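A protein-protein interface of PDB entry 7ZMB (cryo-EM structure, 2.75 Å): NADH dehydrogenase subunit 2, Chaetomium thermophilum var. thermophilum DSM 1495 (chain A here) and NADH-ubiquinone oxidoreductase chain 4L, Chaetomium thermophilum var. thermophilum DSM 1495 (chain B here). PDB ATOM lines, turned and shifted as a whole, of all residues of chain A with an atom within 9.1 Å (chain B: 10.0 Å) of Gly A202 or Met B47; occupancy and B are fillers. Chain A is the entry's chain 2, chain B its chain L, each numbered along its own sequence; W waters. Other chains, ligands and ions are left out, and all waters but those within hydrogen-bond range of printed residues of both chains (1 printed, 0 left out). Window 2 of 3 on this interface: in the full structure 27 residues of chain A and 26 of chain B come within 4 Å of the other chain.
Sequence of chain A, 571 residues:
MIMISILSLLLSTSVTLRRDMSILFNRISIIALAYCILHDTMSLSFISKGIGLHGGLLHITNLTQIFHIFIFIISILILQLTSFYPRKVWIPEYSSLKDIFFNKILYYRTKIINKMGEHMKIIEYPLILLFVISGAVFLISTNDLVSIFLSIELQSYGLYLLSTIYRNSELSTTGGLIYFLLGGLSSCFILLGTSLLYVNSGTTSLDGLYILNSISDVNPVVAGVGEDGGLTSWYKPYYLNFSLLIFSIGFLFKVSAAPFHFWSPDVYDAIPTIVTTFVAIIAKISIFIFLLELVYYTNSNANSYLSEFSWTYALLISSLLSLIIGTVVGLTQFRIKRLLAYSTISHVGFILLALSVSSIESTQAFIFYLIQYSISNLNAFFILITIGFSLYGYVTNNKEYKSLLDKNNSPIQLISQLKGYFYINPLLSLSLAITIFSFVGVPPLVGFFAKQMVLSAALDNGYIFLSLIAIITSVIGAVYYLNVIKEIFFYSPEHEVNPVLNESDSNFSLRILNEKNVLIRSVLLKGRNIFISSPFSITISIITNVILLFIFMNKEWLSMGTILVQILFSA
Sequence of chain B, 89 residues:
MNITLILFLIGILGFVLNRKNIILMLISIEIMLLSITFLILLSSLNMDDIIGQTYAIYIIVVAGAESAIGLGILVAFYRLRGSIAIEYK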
ATOM      1  N   LEU A 145       8.768  -1.792   1.165  1.00  0.00           N
ATOM      2  CA  LEU A 145      10.248  -1.855   1.206  1.00  0.00           C
ATOM      3  C   LEU A 145      10.744  -1.518   2.615  1.00  0.00           C
ATOM      4  O   LEU A 145      11.628  -2.230   3.093  1.00  0.00           O
ATOM      5  CB  LEU A 145      10.821  -0.907   0.152  1.00  0.00           C
ATOM      6  CG  LEU A 145      10.662  -1.362  -1.295  1.00  0.00           C
ATOM      7  CD1 LEU A 145      11.079  -0.260  -2.251  1.00  0.00           C
ATOM      8  CD2 LEU A 145      11.460  -2.631  -1.553  1.00  0.00           C
ATOM      9  N   THR A 194      16.776  -2.107  -1.550  1.00  0.00           N
ATOM     10  CA  THR A 194      15.520  -1.384  -1.379  1.00  0.00           C
ATOM     11  C   THR A 194      15.658   0.067  -1.811  1.00  0.00           C
ATOM     12  O   THR A 194      14.749   0.624  -2.431  1.00  0.00           O
ATOM     13  CB  THR A 194      15.067  -1.450   0.078  1.00  0.00           C
ATOM     14  OG1 THR A 194      16.093  -0.916   0.916  1.00  0.00           O
ATOM     15  CG2 THR A 194      14.777  -2.877   0.505  1.00  0.00           C
ATOM     16  N   SER A 195      16.786   0.695  -1.483  1.00  0.00           N
ATOM     17  CA  SER A 195      16.966   2.111  -1.777  1.00  0.00           C
ATOM     18  C   SER A 195      16.948   2.373  -3.273  1.00  0.00           C
ATOM     19  O   SER A 195      16.406   3.384  -3.722  1.00  0.00           O
ATOM     20  CB  SER A 195      18.265   2.618  -1.152  1.00  0.00           C
ATOM     21  OG  SER A 195      19.400   2.151  -1.849  1.00  0.00           O
ATOM     22  N   LEU A 196      17.531   1.483  -4.064  1.00  0.00           N
ATOM     23  CA  LEU A 196      17.507   1.702  -5.501  1.00  0.00           C
ATOM     24  C   LEU A 196      16.117   1.485  -6.075  1.00  0.00           C
ATOM     25  O   LEU A 196      15.757   2.112  -7.075  1.00  0.00           O
ATOM     26  CB  LEU A 196      18.528   0.800  -6.181  1.00  0.00           C
ATOM     27  CG  LEU A 196      19.963   1.147  -5.794  1.00  0.00           C
ATOM     28  CD1 LEU A 196      20.922   0.086  -6.281  1.00  0.00           C
ATOM     29  CD2 LEU A 196      20.340   2.534  -6.295  1.00  0.00           C
ATOM     30  N   LEU A 197      15.320   0.638  -5.437  1.00  0.00           N
ATOM     31  CA  LEU A 197      13.936   0.411  -5.905  1.00  0.00           C
ATOM     32  C   LEU A 197      13.107   1.683  -5.752  1.00  0.00           C
ATOM     33  O   LEU A 197      12.568   2.119  -6.771  1.00  0.00           O
ATOM     34  CB  LEU A 197      13.323  -0.780  -5.167  1.00  0.00           C
ATOM     35  CG  LEU A 197      13.755  -2.146  -5.692  1.00  0.00           C
ATOM     36  CD1 LEU A 197      13.189  -3.263  -4.838  1.00  0.00           C
ATOM     37  CD2 LEU A 197      13.345  -2.314  -7.145  1.00  0.00           C
ATOM     38  N   TYR A 198      13.080   2.289  -4.562  1.00  0.00           N
ATOM     39  CA  TYR A 198      12.287   3.508  -4.265  1.00  0.00           C
ATOM     40  C   TYR A 198      12.802   4.699  -5.064  1.00  0.00           C
ATOM     41  O   TYR A 198      12.006   5.556  -5.436  1.00  0.00           O
ATOM     42  CB  TYR A 198      12.355   3.808  -2.763  1.00  0.00           C
ATOM     43  CG  TYR A 198      11.974   5.210  -2.373  1.00  0.00           C
ATOM     44  CD1 TYR A 198      10.647   5.594  -2.308  1.00  0.00           C
ATOM     45  CD2 TYR A 198      12.943   6.155  -2.080  1.00  0.00           C
ATOM     46  CE1 TYR A 198      10.292   6.886  -1.964  1.00  0.00           C
ATOM     47  CE2 TYR A 198      12.607   7.450  -1.736  1.00  0.00           C
ATOM     48  CZ  TYR A 198      11.276   7.816  -1.675  1.00  0.00           C
ATOM     49  OH  TYR A 198      10.938   9.090  -1.336  1.00  0.00           O
ATOM     50  N   VAL A 199      14.075   4.699  -5.402  1.00  0.00           N
ATOM     51  CA  VAL A 199      14.694   5.893  -6.030  1.00  0.00           C
ATOM     52  C   VAL A 199      14.350   5.910  -7.518  1.00  0.00           C
ATOM     53  O   VAL A 199      14.074   6.986  -8.058  1.00  0.00           O
ATOM     54  CB  VAL A 199      16.209   5.880  -5.721  1.00  0.00           C
ATOM     55  CG1 VAL A 199      17.088   6.445  -6.810  1.00  0.00           C
ATOM     56  CG2 VAL A 199      16.525   6.487  -4.365  1.00  0.00           C
ATOM     57  N   ASN A 200      14.289   4.730  -8.117  1.00  0.00           N
ATOM     58  CA  ASN A 200      13.930   4.678  -9.528  1.00  0.00           C
ATOM     59  C   ASN A 200      12.434   4.597  -9.762  1.00  0.00           C
ATOM     60  O   ASN A 200      11.976   4.983 -10.837  1.00  0.00           O
ATOM     61  CB  ASN A 200      14.608   3.491 -10.204  1.00  0.00           C
ATOM     62  CG  ASN A 200      16.101   3.628 -10.255  1.00  0.00           C
ATOM     63  OD1 ASN A 200      16.625   4.489 -10.939  1.00  0.00           O
ATOM     64  ND2 ASN A 200      16.797   2.787  -9.516  1.00  0.00           N
ATOM     65  N   SER A 201      11.683   4.121  -8.765  1.00  0.00           N
ATOM     66  CA  SER A 201      10.228   3.883  -8.975  1.00  0.00           C
ATOM     67  C   SER A 201       9.328   4.845  -8.200  1.00  0.00           C
ATOM     68  O   SER A 201       8.129   4.810  -8.484  1.00  0.00           O
ATOM     69  CB  SER A 201       9.903   2.487  -8.550  1.00  0.00           C
ATOM     70  OG  SER A 201      10.018   2.349  -7.145  1.00  0.00           O
ATOM     71  N   GLY A 202       9.844   5.581  -7.215  1.00  0.00           N
ATOM     72  CA  GLY A 202       9.058   6.572  -6.452  1.00  0.00           C
ATOM     73  C   GLY A 202       8.133   5.941  -5.426  1.00  0.00           C
ATOM     74  O   GLY A 202       7.408   6.690  -4.774  1.00  0.00           O
ATOM     75  N   THR A 203       8.187   4.616  -5.246  1.00  0.00           N
ATOM     76  CA  THR A 203       7.225   3.915  -4.366  1.00  0.00           C
ATOM     77  C   THR A 203       7.933   2.978  -3.390  1.00  0.00           C
ATOM     78  O   THR A 203       8.985   2.442  -3.756  1.00  0.00           O
ATOM     79  CB  THR A 203       6.186   3.130  -5.185  1.00  0.00           C
ATOM     80  OG1 THR A 203       5.478   2.241  -4.325  1.00  0.00           O
ATOM     81  CG2 THR A 203       6.781   2.331  -6.323  1.00  0.00           C
ATOM     82  N   THR A 204       7.356   2.802  -2.198  1.00  0.00           N
ATOM     83  CA  THR A 204       7.894   1.834  -1.218  1.00  0.00           C
ATOM     84  C   THR A 204       7.026   0.572  -1.227  1.00  0.00           C
ATOM     85  O   THR A 204       7.450  -0.421  -0.666  1.00  0.00           O
ATOM     86  CB  THR A 204       8.145   2.537   0.120  1.00  0.00           C
ATOM     87  OG1 THR A 204       8.760   1.623   1.024  1.00  0.00           O
ATOM     88  CG2 THR A 204       6.909   3.182   0.707  1.00  0.00           C
ATOM     89  N   SER A 205       5.858   0.618  -1.866  1.00  0.00           N
ATOM     90  CA  SER A 205       4.951  -0.556  -1.970  1.00  0.00           C
ATOM     91  C   SER A 205       5.511  -1.666  -2.847  1.00  0.00           C
ATOM     92  O   SER A 205       5.895  -1.373  -3.982  1.00  0.00           O
ATOM     93  CB  SER A 205       3.593  -0.164  -2.457  1.00  0.00           C
ATOM     94  OG  SER A 205       3.649   0.435  -3.738  1.00  0.00           O
ATOM     95  N   GLY A 208       3.003  -1.892  -5.670  1.00  0.00           N
ATOM     96  CA  GLY A 208       3.245  -0.949  -6.782  1.00  0.00           C
ATOM     97  C   GLY A 208       4.360  -1.378  -7.732  1.00  0.00           C
ATOM     98  O   GLY A 208       4.174  -1.215  -8.941  1.00  0.00           O
ATOM     99  N   LEU A 209       5.475  -1.903  -7.227  1.00  0.00           N
ATOM    100  CA  LEU A 209       6.593  -2.391  -8.074  1.00  0.00           C
ATOM    101  C   LEU A 209       6.160  -3.576  -8.939  1.00  0.00           C
ATOM    102  O   LEU A 209       6.564  -3.626 -10.104  1.00  0.00           O
ATOM    103  CB  LEU A 209       7.761  -2.788  -7.173  1.00  0.00           C
ATOM    104  CG  LEU A 209       8.501  -1.633  -6.499  1.00  0.00           C
ATOM    105  CD1 LEU A 209       9.129  -2.079  -5.188  1.00  0.00           C
ATOM    106  CD2 LEU A 209       9.555  -1.057  -7.426  1.00  0.00           C
ATOM    107  N   LEU A 212       4.200  -2.061 -11.839  1.00  0.00           N
ATOM    108  CA  LEU A 212       5.143  -1.485 -12.833  1.00  0.00           C
ATOM    109  C   LEU A 212       5.816  -2.612 -13.624  1.00  0.00           C
ATOM    110  O   LEU A 212       5.916  -2.484 -14.850  1.00  0.00           O
ATOM    111  CB  LEU A 212       6.190  -0.640 -12.102  1.00  0.00           C
ATOM    112  CG  LEU A 212       5.677   0.631 -11.430  1.00  0.00           C
ATOM    113  CD1 LEU A 212       6.717   1.196 -10.478  1.00  0.00           C
ATOM    114  CD2 LEU A 212       5.288   1.670 -12.466  1.00  0.00           C
ATOM    115  N   TYR A 239      16.217  -1.302 -13.662  1.00  0.00           N
ATOM    116  CA  TYR A 239      16.465  -1.223 -12.203  1.00  0.00           C
ATOM    117  C   TYR A 239      15.821  -2.386 -11.460  1.00  0.00           C
ATOM    118  O   TYR A 239      16.444  -2.828 -10.509  1.00  0.00           O
ATOM    119  CB  TYR A 239      15.996   0.122 -11.640  1.00  0.00           C
ATOM    120  CG  TYR A 239      14.507   0.354 -11.660  1.00  0.00           C
ATOM    121  CD1 TYR A 239      13.865   0.791 -12.806  1.00  0.00           C
ATOM    122  CD2 TYR A 239      13.740   0.153 -10.524  1.00  0.00           C
ATOM    123  CE1 TYR A 239      12.498   1.009 -12.823  1.00  0.00           C
ATOM    124  CE2 TYR A 239      12.374   0.368 -10.524  1.00  0.00           C
ATOM    125  CZ  TYR A 239      11.751   0.800 -11.679  1.00  0.00           C
ATOM    126  OH  TYR A 239      10.405   1.009 -11.686  1.00  0.00           O
ATOM    127  N   LEU B  39      21.435   9.048  -0.408  1.00  0.00           N
ATOM    128  CA  LEU B  39      20.792   8.789  -1.718  1.00  0.00           C
ATOM    129  C   LEU B  39      19.277   8.882  -1.557  1.00  0.00           C
ATOM    130  O   LEU B  39      18.638   9.475  -2.428  1.00  0.00           O
ATOM    131  CB  LEU B  39      21.218   7.430  -2.272  1.00  0.00           C
ATOM    132  CG  LEU B  39      20.518   7.033  -3.565  1.00  0.00           C
ATOM    133  CD1 LEU B  39      20.785   8.065  -4.647  1.00  0.00           C
ATOM    134  CD2 LEU B  39      20.934   5.644  -4.006  1.00  0.00           C
ATOM    135  N   ILE B  40      18.741   8.316  -0.474  1.00  0.00           N
ATOM    136  CA  ILE B  40      17.292   8.331  -0.291  1.00  0.00           C
ATOM    137  C   ILE B  40      16.808   9.745  -0.002  1.00  0.00           C
ATOM    138  O   ILE B  40      15.738  10.156  -0.461  1.00  0.00           O
ATOM    139  CB  ILE B  40      16.895   7.343   0.820  1.00  0.00           C
ATOM    140  CG1 ILE B  40      17.319   5.928   0.428  1.00  0.00           C
ATOM    141  CG2 ILE B  40      15.412   7.386   1.107  1.00  0.00           C
ATOM    142  CD1 ILE B  40      17.512   4.980   1.595  1.00  0.00           C
ATOM    143  N   LEU B  41      17.587  10.516   0.761  1.00  0.00           N
ATOM    144  CA  LEU B  41      17.179  11.884   1.068  1.00  0.00           C
ATOM    145  C   LEU B  41      17.234  12.778  -0.158  1.00  0.00           C
ATOM    146  O   LEU B  41      16.379  13.653  -0.325  1.00  0.00           O
ATOM    147  CB  LEU B  41      18.043  12.469   2.184  1.00  0.00           C
ATOM    148  CG  LEU B  41      17.716  11.985   3.597  1.00  0.00           C
ATOM    149  CD1 LEU B  41      18.861  12.270   4.544  1.00  0.00           C
ATOM    150  CD2 LEU B  41      16.431  12.606   4.102  1.00  0.00           C
ATOM    151  N   LEU B  42      18.217  12.573  -1.030  1.00  0.00           N
ATOM    152  CA  LEU B  42      18.343  13.412  -2.214  1.00  0.00           C
ATOM    153  C   LEU B  42      17.267  13.109  -3.249  1.00  0.00           C
ATOM    154  O   LEU B  42      16.725  14.028  -3.864  1.00  0.00           O
ATOM    155  CB  LEU B  42      19.737  13.251  -2.807  1.00  0.00           C
ATOM    156  CG  LEU B  42      20.729  14.144  -2.068  1.00  0.00           C
ATOM    157  CD1 LEU B  42      22.158  13.777  -2.386  1.00  0.00           C
ATOM    158  CD2 LEU B  42      20.452  15.564  -2.446  1.00  0.00           C
ATOM    159  N   SER B  43      16.947  11.837  -3.464  1.00  0.00           N
ATOM    160  CA  SER B  43      15.817  11.411  -4.338  1.00  0.00           C
ATOM    161  C   SER B  43      14.475  11.949  -3.846  1.00  0.00           C
ATOM    162  O   SER B  43      13.714  12.463  -4.664  1.00  0.00           O
ATOM    163  CB  SER B  43      15.793   9.932  -4.467  1.00  0.00           C
ATOM    164  OG  SER B  43      16.966   9.492  -5.131  1.00  0.00           O
ATOM    165  N   SER B  44      14.192  11.815  -2.565  1.00  0.00           N
ATOM    166  CA  SER B  44      12.907  12.270  -1.992  1.00  0.00           C
ATOM    167  C   SER B  44      12.681  13.768  -2.227  1.00  0.00           C
ATOM    168  O   SER B  44      11.509  14.157  -2.363  1.00  0.00           O
ATOM    169  CB  SER B  44      12.887  11.919  -0.554  1.00  0.00           C
ATOM    170  OG  SER B  44      13.340  10.593  -0.405  1.00  0.00           O
ATOM    171  N   LEU B  45      13.729  14.586  -2.241  1.00  0.00           N
ATOM    172  CA  LEU B  45      13.553  16.032  -2.513  1.00  0.00           C
ATOM    173  C   LEU B  45      13.204  16.229  -3.981  1.00  0.00           C
ATOM    174  O   LEU B  45      12.353  17.061  -4.266  1.00  0.00           O
ATOM    175  CB  LEU B  45      14.870  16.713  -2.134  1.00  0.00           C
ATOM    176  CG  LEU B  45      15.009  18.193  -2.484  1.00  0.00           C
ATOM    177  CD1 LEU B  45      14.001  19.033  -1.716  1.00  0.00           C
ATOM    178  CD2 LEU B  45      16.420  18.669  -2.198  1.00  0.00           C
ATOM    179  N   ASN B  46      13.801  15.450  -4.861  1.00  0.00           N
ATOM    180  CA  ASN B  46      13.512  15.491  -6.322  1.00  0.00           C
ATOM    181  C   ASN B  46      12.086  15.031  -6.633  1.00  0.00           C
ATOM    182  O   ASN B  46      11.529  15.519  -7.615  1.00  0.00           O
ATOM    183  CB  ASN B  46      14.533  14.646  -7.078  1.00  0.00           C
ATOM    184  CG  ASN B  46      15.961  15.128  -6.942  1.00  0.00           C
ATOM    185  OD1 ASN B  46      16.892  14.392  -7.249  1.00  0.00           O
ATOM    186  ND2 ASN B  46      16.147  16.353  -6.483  1.00  0.00           N
ATOM    187  N   MET B  47      11.543  14.075  -5.875  1.00  0.00           N
ATOM    188  CA  MET B  47      10.195  13.513  -6.153  1.00  0.00           C
ATOM    189  C   MET B  47       9.129  14.057  -5.199  1.00  0.00           C
ATOM    190  O   MET B  47       8.055  13.458  -5.176  1.00  0.00           O
ATOM    191  CB  MET B  47      10.221  11.988  -6.082  1.00  0.00           C
ATOM    192  CG  MET B  47      11.402  11.380  -6.808  1.00  0.00           C
ATOM    193  SD  MET B  47      11.396   9.577  -6.793  1.00  0.00           S
ATOM    194  CE  MET B  47      11.933   9.222  -5.121  1.00  0.00           C
ATOM    195  N   ASP B  48       9.394  15.121  -4.439  1.00  0.00           N
ATOM    196  CA  ASP B  48       8.382  15.742  -3.530  1.00  0.00           C
ATOM    197  C   ASP B  48       7.812  14.683  -2.577  1.00  0.00           C
ATOM    198  O   ASP B  48       6.599  14.650  -2.419  1.00  0.00           O
ATOM    199  CB  ASP B  48       7.361  16.584  -4.306  1.00  0.00           C
ATOM    200  CG  ASP B  48       6.420  17.405  -3.438  1.00  0.00           C
ATOM    201  OD1 ASP B  48       5.225  17.472  -3.781  1.00  0.00           O
ATOM    202  OD2 ASP B  48       6.888  17.973  -2.430  1.00  0.00           O
ATOM    203  N   ASP B  49       8.639  13.801  -2.017  1.00  0.00           N
ATOM    204  CA  ASP B  49       8.110  12.686  -1.196  1.00  0.00           C
ATOM    205  C   ASP B  49       8.561  12.842   0.256  1.00  0.00           C
ATOM    206  O   ASP B  49       9.773  12.887   0.502  1.00  0.00           O
ATOM    207  CB  ASP B  49       8.587  11.353  -1.759  1.00  0.00           C
ATOM    208  CG  ASP B  49       7.738  10.179  -1.294  1.00  0.00           C
ATOM    209  OD1 ASP B  49       6.746  10.416  -0.587  1.00  0.00           O
ATOM    210  OD2 ASP B  49       8.073   9.038  -1.644  1.00  0.00           O
ATOM    211  N   ILE B  50       7.615  12.897   1.184  1.00  0.00           N
ATOM    212  CA  ILE B  50       8.004  12.958   2.616  1.00  0.00           C
ATOM    213  C   ILE B  50       8.348  11.532   3.070  1.00  0.00           C
ATOM    214  O   ILE B  50       8.970  11.387   4.127  1.00  0.00           O
ATOM    215  CB  ILE B  50       6.919  13.683   3.449  1.00  0.00           C
ATOM    216  CG1 ILE B  50       7.496  14.364   4.690  1.00  0.00           C
ATOM    217  CG2 ILE B  50       5.762  12.765   3.783  1.00  0.00           C
ATOM    218  CD1 ILE B  50       8.663  15.273   4.408  1.00  0.00           C
ATOM    219  N   ILE B  51       7.952  10.527   2.291  1.00  0.00           N
ATOM    220  CA  ILE B  51       8.174   9.103   2.682  1.00  0.00           C
ATOM    221  C   ILE B  51       9.664   8.802   2.697  1.00  0.00           C
ATOM    222  O   ILE B  51      10.098   8.065   3.583  1.00  0.00           O
ATOM    223  CB  ILE B  51       7.330   8.117   1.840  1.00  0.00           C
ATOM    224  CG1 ILE B  51       5.855   8.226   2.220  1.00  0.00           C
ATOM    225  CG2 ILE B  51       7.826   6.686   1.963  1.00  0.00           C
ATOM    226  CD1 ILE B  51       5.646   8.451   3.684  1.00  0.00           C
ATOM    227  N   GLY B  52      10.411   9.363   1.760  1.00  0.00           N
ATOM    228  CA  GLY B  52      11.869   9.172   1.748  1.00  0.00           C
ATOM    229  C   GLY B  52      12.547   9.733   2.968  1.00  0.00           C
ATOM    230  O   GLY B  52      13.486   9.099   3.437  1.00  0.00           O
ATOM    231  N   GLN B  53      12.134  10.904   3.442  1.00  0.00           N
ATOM    232  CA  GLN B  53      12.695  11.443   4.710  1.00  0.00           C
ATOM    233  C   GLN B  53      12.273  10.547   5.864  1.00  0.00           C
ATOM    234  O   GLN B  53      13.073  10.368   6.783  1.00  0.00           O
ATOM    235  CB  GLN B  53      12.320  12.902   4.946  1.00  0.00           C
ATOM    236  CG  GLN B  53      12.811  13.858   3.870  1.00  0.00           C
ATOM    237  CD  GLN B  53      12.623  15.290   4.305  1.00  0.00           C
ATOM    238  OE1 GLN B  53      12.586  15.597   5.492  1.00  0.00           O
ATOM    239  NE2 GLN B  53      12.503  16.182   3.338  1.00  0.00           N
ATOM    240  N   TYR B  55      11.680   7.328   5.614  1.00  0.00           N
ATOM    241  CA  TYR B  55      12.551   6.171   5.465  1.00  0.00           C
ATOM    242  C   TYR B  55      13.953   6.476   5.966  1.00  0.00           C
ATOM    243  O   TYR B  55      14.580   5.640   6.625  1.00  0.00           O
ATOM    244  CB  TYR B  55      12.570   5.735   3.999  1.00  0.00           C
ATOM    245  CG  TYR B  55      13.253   4.415   3.720  1.00  0.00           C
ATOM    246  CD1 TYR B  55      13.428   3.478   4.722  1.00  0.00           C
ATOM    247  CD2 TYR B  55      13.629   4.069   2.432  1.00  0.00           C
ATOM    248  CE1 TYR B  55      14.016   2.275   4.475  1.00  0.00           C
ATOM    249  CE2 TYR B  55      14.218   2.860   2.170  1.00  0.00           C
ATOM    250  CZ  TYR B  55      14.406   1.962   3.201  1.00  0.00           C
ATOM    251  OH  TYR B  55      14.986   0.743   2.972  1.00  0.00           O
HETATM  252  O   HOH W   1       6.073   6.443  -2.079  1.00  0.00           O
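Ser A195 touches Ile B40.
CD2 of Leu B39 touches CD2 of Leu A196 (3.9 Å).
Tyr A198 touches Ile B40.
Tyr A198 touches Met B47 (O to CE, 3.7 Å).
Ser B43 touches Val A199 (OG to CG2, 3.1 Å).
O of Val A199 touches SD of Met B47, at 3.9 Å.
Met B47 touches Gly A202.
Gly A202 touches Asp B49.
Thr A204 touches Ile B51.
Of the printed residues of chain B, Ser A195 touches Ile B40.
Of the printed residues of chain B, Val A199 touches Ser B43 (3.1 Å) and Met B47 (3.9 Å).
No residue of chain B comes within 4 Å of Ser A201.
Of chain B, only Met B47 and Asp B49 come within 4 Å of Gly A202.
Thr A203 touches none of the printed residues of chain B.
Of chain A, only Tyr A198, Val A199 and Gly A202 come within 4 Å of Met B47.
OD1 of Asp B49 is in hydrogen-bond range of N of Ile B51, 3.1 Å away.
The backbone carbonyl oxygen of Leu B39 is in hydrogen-bond range of the side-chain hydroxyl of Ser B43 (3.2 Å).
The backbone carbonyl oxygen (O) of Leu A196 lies within hydrogen-bond range of the side-chain amide nitrogen (ND2) of Asn A200, at 2.7 Å.
O of Ile B40 is in hydrogen-bond range of OG of Ser B44, at 2.4 Å.
The backbone carbonyl oxygen (O) of Ser B44 lies within hydrogen-bond range of the backbone NH (N) of Asp B49, 2.9 Å away.
O of Thr A204 lies within hydrogen-bond range of N of Leu A145 (2.6 Å).
Water W1 lies within hydrogen-bond range of the backbone carbonyl oxygen of Gly A202 (3.0 Å) and the side-chain carboxylate of Asp B49 (3.3 Å).
OH of Tyr A198 is in hydrogen-bond range of OD2 of Asp B49 (2.9 Å).
OH of Tyr A198 is in hydrogen-bond range of N of Gly B52, at 3.2 Å.
OH of Tyr A198 lies within hydrogen-bond range of OG of Ser B44.
The side-chain hydroxyl (OH) of Tyr B55 sits at hydrogen-bond distance from the side-chain hydroxyl (OG1) of Thr A194 (2.9 Å).
Of the 17 printed residues of chain A, 7 touch a printed residue of chain B.
Of the 16 printed residues of chain B, 9 touch a printed residue of chain A.
Printed residues of chain B that touch a printed residue of chain A: Leu B39, Ile B40, Ser B43, Ser B44, Met B47, Asp B49, Ile B51, Gly B52 and Tyr B55.
Hydrophobic or aromatic side chains of chain B within 4 Å of the printed part of chain A: Leu B39, Ile B40, Met B47, Ile B51 and Tyr B55.
Among the printed residues, 13 pairs touch across the chains.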
